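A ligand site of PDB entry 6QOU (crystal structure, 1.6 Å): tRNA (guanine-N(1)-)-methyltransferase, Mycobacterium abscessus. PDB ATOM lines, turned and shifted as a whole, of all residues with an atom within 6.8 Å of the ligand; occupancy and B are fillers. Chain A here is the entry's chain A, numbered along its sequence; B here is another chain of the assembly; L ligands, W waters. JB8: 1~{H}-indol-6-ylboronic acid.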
ATOM      1  N   MET A  63     -10.592  26.961  11.026  1.00  0.00           N
ATOM      2  CA  MET A  63     -11.554  27.866  10.393  1.00  0.00           C
ATOM      3  C   MET A  63     -12.612  28.376  11.387  1.00  0.00           C
ATOM      4  O   MET A  63     -13.081  27.633  12.262  1.00  0.00           O
ATOM      5  CB  MET A  63     -12.198  27.184   9.181  1.00  0.00           C
ATOM      6  CG  MET A  63     -11.175  26.794   8.110  1.00  0.00           C
ATOM      7  SD  MET A  63     -11.928  26.397   6.492  1.00  0.00           S
ATOM      8  CE  MET A  63     -11.509  27.859   5.545  1.00  0.00           C
ATOM      9  N   VAL A  84     -19.386  16.921   5.276  1.00  0.00           N
ATOM     10  CA  VAL A  84     -18.141  17.592   5.670  1.00  0.00           C
ATOM     11  C   VAL A  84     -16.941  16.653   5.439  1.00  0.00           C
ATOM     12  O   VAL A  84     -16.687  15.747   6.264  1.00  0.00           O
ATOM     13  CB  VAL A  84     -18.143  18.020   7.166  1.00  0.00           C
ATOM     14  CG1 VAL A  84     -16.902  18.816   7.497  1.00  0.00           C
ATOM     15  CG2 VAL A  84     -19.415  18.814   7.512  1.00  0.00           C
ATOM     16  N   PRO A  85     -16.207  16.823   4.323  1.00  0.00           N
ATOM     17  CA  PRO A  85     -15.020  15.980   4.127  1.00  0.00           C
ATOM     18  C   PRO A  85     -13.957  16.245   5.193  1.00  0.00           C
ATOM     19  O   PRO A  85     -13.688  17.408   5.522  1.00  0.00           O
ATOM     20  CB  PRO A  85     -14.511  16.368   2.730  1.00  0.00           C
ATOM     21  CG  PRO A  85     -15.766  16.913   2.006  1.00  0.00           C
ATOM     22  CD  PRO A  85     -16.517  17.630   3.124  1.00  0.00           C
ATOM     23  N   THR A  86     -13.357  15.169   5.710  1.00  0.00           N
ATOM     24  CA  THR A  86     -12.298  15.271   6.716  1.00  0.00           C
ATOM     25  C   THR A  86     -11.552  13.934   6.809  1.00  0.00           C
ATOM     26  O   THR A  86     -12.185  12.874   6.692  1.00  0.00           O
ATOM     27  CB  THR A  86     -12.857  15.682   8.126  1.00  0.00           C
ATOM     28  OG1 THR A  86     -11.871  15.420   9.142  1.00  0.00           O
ATOM     29  CG2 THR A  86     -14.151  14.945   8.467  1.00  0.00           C
ATOM     30  N   PRO A  87     -10.234  13.969   7.020  1.00  0.00           N
ATOM     31  CA  PRO A  87      -9.485  12.703   7.138  1.00  0.00           C
ATOM     32  C   PRO A  87      -9.893  11.947   8.391  1.00  0.00           C
ATOM     33  O   PRO A  87      -9.587  10.752   8.489  1.00  0.00           O
ATOM     34  CB  PRO A  87      -8.010  13.150   7.199  1.00  0.00           C
ATOM     35  CG  PRO A  87      -8.045  14.577   7.634  1.00  0.00           C
ATOM     36  CD  PRO A  87      -9.380  15.155   7.206  1.00  0.00           C
ATOM     37  N   ALA A  88     -10.600  12.611   9.308  1.00  0.00           N
ATOM     38  CA  ALA A  88     -11.080  11.952  10.519  1.00  0.00           C
ATOM     39  C   ALA A  88     -12.531  11.473  10.418  1.00  0.00           C
ATOM     40  O   ALA A  88     -13.163  11.166  11.435  1.00  0.00           O
ATOM     41  CB  ALA A  88     -10.926  12.908  11.720  1.00  0.00           C
ATOM     42  N   ALA A 109     -19.407  21.200   2.735  1.00  0.00           N
ATOM     43  CA  ALA A 109     -18.597  22.233   3.381  1.00  0.00           C
ATOM     44  C   ALA A 109     -17.120  21.876   3.283  1.00  0.00           C
ATOM     45  O   ALA A 109     -16.657  20.962   3.967  1.00  0.00           O
ATOM     46  CB  ALA A 109     -19.012  22.392   4.870  1.00  0.00           C
ATOM     47  N   CYS A 110     -16.375  22.614   2.454  1.00  0.00           N
ATOM     48  CA  CYS A 110     -14.942  22.325   2.225  1.00  0.00           C
ATOM     49  C   CYS A 110     -14.027  23.105   3.157  1.00  0.00           C
ATOM     50  O   CYS A 110     -13.941  24.339   3.069  1.00  0.00           O
ATOM     51  CB  CYS A 110     -14.558  22.620   0.770  1.00  0.00           C
ATOM     52  SG  CYS A 110     -15.425  21.650  -0.501  1.00  0.00           S
ATOM     53  N   GLY A 111     -13.300  22.398   4.021  1.00  0.00           N
ATOM     54  CA  GLY A 111     -12.337  23.021   4.908  1.00  0.00           C
ATOM     55  C   GLY A 111     -10.934  23.085   4.355  1.00  0.00           C
ATOM     56  O   GLY A 111     -10.627  22.506   3.293  1.00  0.00           O
ATOM     57  N   ARG A 112     -10.086  23.805   5.096  1.00  0.00           N
ATOM     58  CA  ARG A 112      -8.670  24.013   4.784  1.00  0.00           C
ATOM     59  C   ARG A 112      -7.917  24.112   6.102  1.00  0.00           C
ATOM     60  O   ARG A 112      -8.521  24.028   7.175  1.00  0.00           O
ATOM     61  CB  ARG A 112      -8.460  25.287   3.946  1.00  0.00           C
ATOM     62  CG  ARG A 112      -8.800  25.135   2.444  1.00  0.00           C
ATOM     63  CD  ARG A 112      -7.561  24.774   1.627  1.00  0.00           C
ATOM     64  NE  ARG A 112      -7.882  24.011   0.422  1.00  0.00           N
ATOM     65  CZ  ARG A 112      -6.984  23.617  -0.480  1.00  0.00           C
ATOM     66  NH1 ARG A 112      -5.707  23.939  -0.315  1.00  0.00           N
ATOM     67  NH2 ARG A 112      -7.364  22.924  -1.546  1.00  0.00           N
ATOM     68  N   TYR A 113      -6.599  24.297   6.021  1.00  0.00           N
ATOM     69  CA  TYR A 113      -5.742  24.365   7.207  1.00  0.00           C
ATOM     70  C   TYR A 113      -5.938  23.121   8.078  1.00  0.00           C
ATOM     71  O   TYR A 113      -5.859  21.996   7.585  1.00  0.00           O
ATOM     72  CB  TYR A 113      -6.028  25.636   8.031  1.00  0.00           C
ATOM     73  CG  TYR A 113      -6.161  26.898   7.209  1.00  0.00           C
ATOM     74  CD1 TYR A 113      -5.038  27.608   6.788  1.00  0.00           C
ATOM     75  CD2 TYR A 113      -7.414  27.407   6.885  1.00  0.00           C
ATOM     76  CE1 TYR A 113      -5.161  28.772   6.052  1.00  0.00           C
ATOM     77  CE2 TYR A 113      -7.546  28.567   6.148  1.00  0.00           C
ATOM     78  CZ  TYR A 113      -6.418  29.244   5.736  1.00  0.00           C
ATOM     79  OH  TYR A 113      -6.551  30.403   5.008  1.00  0.00           O
ATOM     80  N   GLU A 114      -6.248  23.307   9.358  1.00  0.00           N
ATOM     81  CA  GLU A 114      -6.425  22.167  10.247  1.00  0.00           C
ATOM     82  C   GLU A 114      -7.897  21.823  10.515  1.00  0.00           C
ATOM     83  O   GLU A 114      -8.218  21.107  11.457  1.00  0.00           O
ATOM     84  CB  GLU A 114      -5.688  22.418  11.563  1.00  0.00           C
ATOM     85  CG  GLU A 114      -4.204  22.744  11.366  1.00  0.00           C
ATOM     86  CD  GLU A 114      -3.520  21.734  10.445  1.00  0.00           C
ATOM     87  OE1 GLU A 114      -3.027  22.135   9.371  1.00  0.00           O
ATOM     88  OE2 GLU A 114      -3.471  20.542  10.811  1.00  0.00           O
ATOM     89  N   GLY A 115      -8.786  22.323   9.663  1.00  0.00           N
ATOM     90  CA  GLY A 115     -10.202  21.967   9.734  1.00  0.00           C
ATOM     91  C   GLY A 115     -11.117  23.066  10.275  1.00  0.00           C
ATOM     92  O   GLY A 115     -10.653  24.168  10.528  1.00  0.00           O
ATOM     93  N   ILE A 116     -12.394  22.742  10.462  1.00  0.00           N
ATOM     94  CA  ILE A 116     -13.424  23.708  10.873  1.00  0.00           C
ATOM     95  C   ILE A 116     -13.733  23.536  12.372  1.00  0.00           C
ATOM     96  O   ILE A 116     -13.828  22.410  12.838  1.00  0.00           O
ATOM     97  CB  ILE A 116     -14.724  23.537  10.061  1.00  0.00           C
ATOM     98  CG1 ILE A 116     -14.406  23.575   8.544  1.00  0.00           C
ATOM     99  CG2 ILE A 116     -15.784  24.577  10.463  1.00  0.00           C
ATOM    100  CD1 ILE A 116     -15.595  23.227   7.651  1.00  0.00           C
ATOM    101  N   VAL A 133     -17.049  12.721   6.588  1.00  0.00           N
ATOM    102  CA  VAL A 133     -16.589  11.537   5.827  1.00  0.00           C
ATOM    103  C   VAL A 133     -15.188  11.669   5.257  1.00  0.00           C
ATOM    104  O   VAL A 133     -14.770  12.748   4.820  1.00  0.00           O
ATOM    105  CB  VAL A 133     -17.541  11.186   4.645  1.00  0.00           C
ATOM    106  CG1 VAL A 133     -18.872  10.658   5.157  1.00  0.00           C
ATOM    107  CG2 VAL A 133     -17.744  12.375   3.701  1.00  0.00           C
ATOM    108  N   SER A 134     -14.477  10.543   5.239  1.00  0.00           N
ATOM    109  CA  SER A 134     -13.169  10.427   4.595  1.00  0.00           C
ATOM    110  C   SER A 134     -13.249   9.606   3.299  1.00  0.00           C
ATOM    111  O   SER A 134     -13.797   8.490   3.308  1.00  0.00           O
ATOM    112  CB  SER A 134     -12.155   9.768   5.530  1.00  0.00           C
ATOM    113  OG  SER A 134     -10.949   9.456   4.844  1.00  0.00           O
ATOM    114  N   ILE A 135     -12.678  10.120   2.208  1.00  0.00           N
ATOM    115  CA  ILE A 135     -12.702   9.377   0.943  1.00  0.00           C
ATOM    116  C   ILE A 135     -11.572   8.340   0.789  1.00  0.00           C
ATOM    117  O   ILE A 135     -11.557   7.561  -0.183  1.00  0.00           O
ATOM    118  CB  ILE A 135     -12.668  10.323  -0.305  1.00  0.00           C
ATOM    119  CG1 ILE A 135     -11.395  11.184  -0.329  1.00  0.00           C
ATOM    120  CG2 ILE A 135     -13.949  11.171  -0.389  1.00  0.00           C
ATOM    121  CD1 ILE A 135     -11.065  11.713  -1.765  1.00  0.00           C
ATOM    122  N   GLY A 136     -10.626   8.310   1.726  1.00  0.00           N
ATOM    123  CA  GLY A 136      -9.559   7.329   1.720  1.00  0.00           C
ATOM    124  C   GLY A 136      -8.540   7.603   2.813  1.00  0.00           C
ATOM    125  O   GLY A 136      -8.600   8.659   3.455  1.00  0.00           O
ATOM    126  N   TYR A 138      -5.606   8.865   3.389  1.00  0.00           N
ATOM    127  CA  TYR A 138      -4.539   9.783   3.026  1.00  0.00           C
ATOM    128  C   TYR A 138      -5.008  11.195   3.398  1.00  0.00           C
ATOM    129  O   TYR A 138      -6.219  11.460   3.537  1.00  0.00           O
ATOM    130  CB  TYR A 138      -4.186   9.715   1.526  1.00  0.00           C
ATOM    131  CG  TYR A 138      -5.411   9.507   0.659  1.00  0.00           C
ATOM    132  CD1 TYR A 138      -6.272  10.561   0.367  1.00  0.00           C
ATOM    133  CD2 TYR A 138      -5.731   8.247   0.168  1.00  0.00           C
ATOM    134  CE1 TYR A 138      -7.419  10.373  -0.391  1.00  0.00           C
ATOM    135  CE2 TYR A 138      -6.858   8.047  -0.609  1.00  0.00           C
ATOM    136  CZ  TYR A 138      -7.703   9.110  -0.879  1.00  0.00           C
ATOM    137  OH  TYR A 138      -8.841   8.904  -1.627  1.00  0.00           O
ATOM    138  N   VAL A 139      -4.029  12.084   3.558  1.00  0.00           N
ATOM    139  CA  VAL A 139      -4.274  13.472   3.920  1.00  0.00           C
ATOM    140  C   VAL A 139      -4.131  14.399   2.712  1.00  0.00           C
ATOM    141  O   VAL A 139      -3.111  14.373   2.025  1.00  0.00           O
ATOM    142  CB  VAL A 139      -3.317  13.930   5.039  1.00  0.00           C
ATOM    143  CG1 VAL A 139      -3.507  15.419   5.332  1.00  0.00           C
ATOM    144  CG2 VAL A 139      -3.544  13.116   6.306  1.00  0.00           C
ATOM    145  N   LEU A 140      -5.166  15.204   2.438  1.00  0.00           N
ATOM    146  CA  LEU A 140      -5.104  16.234   1.410  1.00  0.00           C
ATOM    147  C   LEU A 140      -4.877  17.624   2.040  1.00  0.00           C
ATOM    148  O   LEU A 140      -4.872  17.736   3.265  1.00  0.00           O
ATOM    149  CB  LEU A 140      -6.398  16.238   0.588  1.00  0.00           C
ATOM    150  CG  LEU A 140      -6.789  14.881   0.005  1.00  0.00           C
ATOM    151  CD1 LEU A 140      -8.191  14.915  -0.564  1.00  0.00           C
ATOM    152  CD2 LEU A 140      -5.795  14.462  -1.071  1.00  0.00           C
ATOM    153  N   ASN A 141      -4.713  18.665   1.233  1.00  0.00           N
ATOM    154  CA  ASN A 141      -4.581  20.037   1.783  1.00  0.00           C
ATOM    155  C   ASN A 141      -5.916  20.633   2.232  1.00  0.00           C
ATOM    156  O   ASN A 141      -5.962  21.534   3.087  1.00  0.00           O
ATOM    157  CB  ASN A 141      -3.955  20.973   0.743  1.00  0.00           C
ATOM    158  CG  ASN A 141      -2.477  20.721   0.531  1.00  0.00           C
ATOM    159  OD1 ASN A 141      -1.747  20.361   1.456  1.00  0.00           O
ATOM    160  ND2 ASN A 141      -2.024  20.905  -0.702  1.00  0.00           N
ATOM    161  N   GLY A 142      -7.012  20.151   1.652  1.00  0.00           N
ATOM    162  CA  GLY A 142      -8.334  20.653   1.966  1.00  0.00           C
ATOM    163  C   GLY A 142      -9.408  19.769   1.364  1.00  0.00           C
ATOM    164  O   GLY A 142      -9.104  18.749   0.737  1.00  0.00           O
ATOM    165  N   GLY A 143     -10.662  20.160   1.556  1.00  0.00           N
ATOM    166  CA  GLY A 143     -11.781  19.307   1.163  1.00  0.00           C
ATOM    167  C   GLY A 143     -12.229  19.313  -0.289  1.00  0.00           C
ATOM    168  O   GLY A 143     -13.076  18.489  -0.674  1.00  0.00           O
ATOM    169  N   GLU A 144     -11.663  20.203  -1.116  1.00  0.00           N
ATOM    170  CA  GLU A 144     -12.150  20.382  -2.492  1.00  0.00           C
ATOM    171  C   GLU A 144     -12.018  19.138  -3.400  1.00  0.00           C
ATOM    172  O   GLU A 144     -12.974  18.783  -4.099  1.00  0.00           O
ATOM    173  CB  GLU A 144     -11.406  21.567  -3.132  1.00  0.00           C
ATOM    174  CG  GLU A 144     -11.845  22.947  -2.588  1.00  0.00           C
ATOM    175  CD  GLU A 144     -11.240  23.319  -1.238  1.00  0.00           C
ATOM    176  OE1 GLU A 144     -10.301  22.654  -0.753  1.00  0.00           O
ATOM    177  OE2 GLU A 144     -11.718  24.310  -0.650  1.00  0.00           O
ATOM    178  N   ALA A 146     -11.862  16.071  -2.444  1.00  0.00           N
ATOM    179  CA  ALA A 146     -12.842  15.120  -1.893  1.00  0.00           C
ATOM    180  C   ALA A 146     -14.279  15.433  -2.347  1.00  0.00           C
ATOM    181  O   ALA A 146     -15.060  14.520  -2.680  1.00  0.00           O
ATOM    182  CB  ALA A 146     -12.754  15.093  -0.346  1.00  0.00           C
ATOM    183  N   GLU B 152      -2.448  15.799  -5.332  1.00  0.00           N
ATOM    184  CA  GLU B 152      -2.459  16.591  -4.097  1.00  0.00           C
ATOM    185  C   GLU B 152      -1.827  15.852  -2.903  1.00  0.00           C
ATOM    186  O   GLU B 152      -1.050  16.451  -2.166  1.00  0.00           O
ATOM    187  CB  GLU B 152      -3.888  17.008  -3.749  1.00  0.00           C
ATOM    188  CG  GLU B 152      -3.934  17.931  -2.550  1.00  0.00           C
ATOM    189  CD  GLU B 152      -5.258  18.662  -2.414  1.00  0.00           C
ATOM    190  OE1 GLU B 152      -5.976  18.799  -3.432  1.00  0.00           O
ATOM    191  OE2 GLU B 152      -5.585  19.079  -1.293  1.00  0.00           O
HETATM  192  C10 JB8 L   1      -8.120  20.387   5.765  1.00  0.00           C
HETATM  193  O01 JB8 L   1      -7.583  14.136   3.505  1.00  0.00           O
HETATM  194  B02 JB8 L   1      -8.880  14.734   3.314  1.00  0.00           B
HETATM  195  C03 JB8 L   1      -9.157  16.264   3.913  1.00  0.00           C
HETATM  196  C04 JB8 L   1      -8.077  17.048   4.369  1.00  0.00           C
HETATM  197  C05 JB8 L   1      -8.316  18.348   4.887  1.00  0.00           C
HETATM  198  C06 JB8 L   1      -9.603  18.847   4.953  1.00  0.00           C
HETATM  199  C07 JB8 L   1     -10.691  18.058   4.486  1.00  0.00           C
HETATM  200  C08 JB8 L   1     -10.457  16.768   3.967  1.00  0.00           C
HETATM  201  C09 JB8 L   1      -9.479  20.168   5.518  1.00  0.00           C
HETATM  202  N11 JB8 L   1      -7.450  19.297   5.382  1.00  0.00           N
HETATM  203  O12 JB8 L   1      -9.985  13.819   3.251  1.00  0.00           O
HETATM  204  O   HOH W   1     -12.760  13.120   2.644  1.00  0.00           O
HETATM  205  O   HOH W   2      -9.322  11.367   3.247  1.00  0.00           O
HETATM  206  O   HOH W   3      -4.542  18.946   5.817  1.00  0.00           O
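The backbone NH (N) of Leu 140 is in hydrogen-bond range of an oxygen (O01) of the ligand, 2.8 Å away.
O of Tyr 138 sits at hydrogen-bond distance from O01 of the ligand, 3.0 Å away.
O of Ile 135 lies within hydrogen-bond range of OH of Tyr 138, at 3.4 Å.
The backbone NH (N) of Gly 143 sits at hydrogen-bond distance from the backbone carbonyl oxygen (O) of Gly 111 (2.9 Å).
The backbone NH (N) of Asn 141 lies within hydrogen-bond range of the side-chain carboxylate (OE2) of Glu 152 of chain B.
The backbone NH of Thr 86 lies within hydrogen-bond range of the backbone carbonyl oxygen of Val 133 (2.9 Å).
The backbone NH (N) of Ala 88 lies close to the side-chain hydroxyl (OG1) of Thr 86, 3.1 Å away.
N of Gly 142 is in hydrogen-bond range of OE2 of Glu 152 of chain B (3.4 Å).
The guanidinium group of Arg 112 is in salt-bridge range of the side-chain carboxylate of Glu 144.
The backbone NH of Arg 112 is in hydrogen-bond range of the side-chain sulfur of Met 63.
Pro 85 touches the ligand (O to C07, 3.2 Å).
Thr 86 touches the ligand (CA to C08, 3.6 Å).
CD of Pro 87 touches C03 of the ligand, 3.5 Å away.
Gly 111 touches the ligand.
N of Arg 112 touches C09 of the ligand, at 3.7 Å.
Tyr 113 touches the ligand (O to C10, 3.3 Å).
CA of Val 139 touches O01 of the ligand, at 3.4 Å.
Asn 141 touches the ligand.
Gly 142 touches the ligand (C to C06, 3.7 Å).
N of Gly 143 touches C07 of the ligand, at 3.6 Å.
Of the 27 residues printed, 12 come within 4 Å of the ligand.
The nearest printed residue that does not touch the ligand is Gly 115 (4.4 Å).
Water W2 lies within hydrogen-bond range of an oxygen (O12) of the ligand (2.5 Å), the backbone carbonyl oxygen of Gly 136 (2.8 Å), the side-chain hydroxyl of Ser 134 (3.0 Å) and the backbone carbonyl oxygen of Tyr 138 (3.1 Å).
Water W1 lies within hydrogen-bond range of an oxygen (O12) of the ligand (2.9 Å), the backbone carbonyl oxygen (O) of Val 133 (3.0 Å) and the backbone NH (N) of Ile 135 (3.0 Å).
Water W3 lies within hydrogen-bond range of O of Leu 140 (2.8 Å) and N11 of the ligand (3.0 Å).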
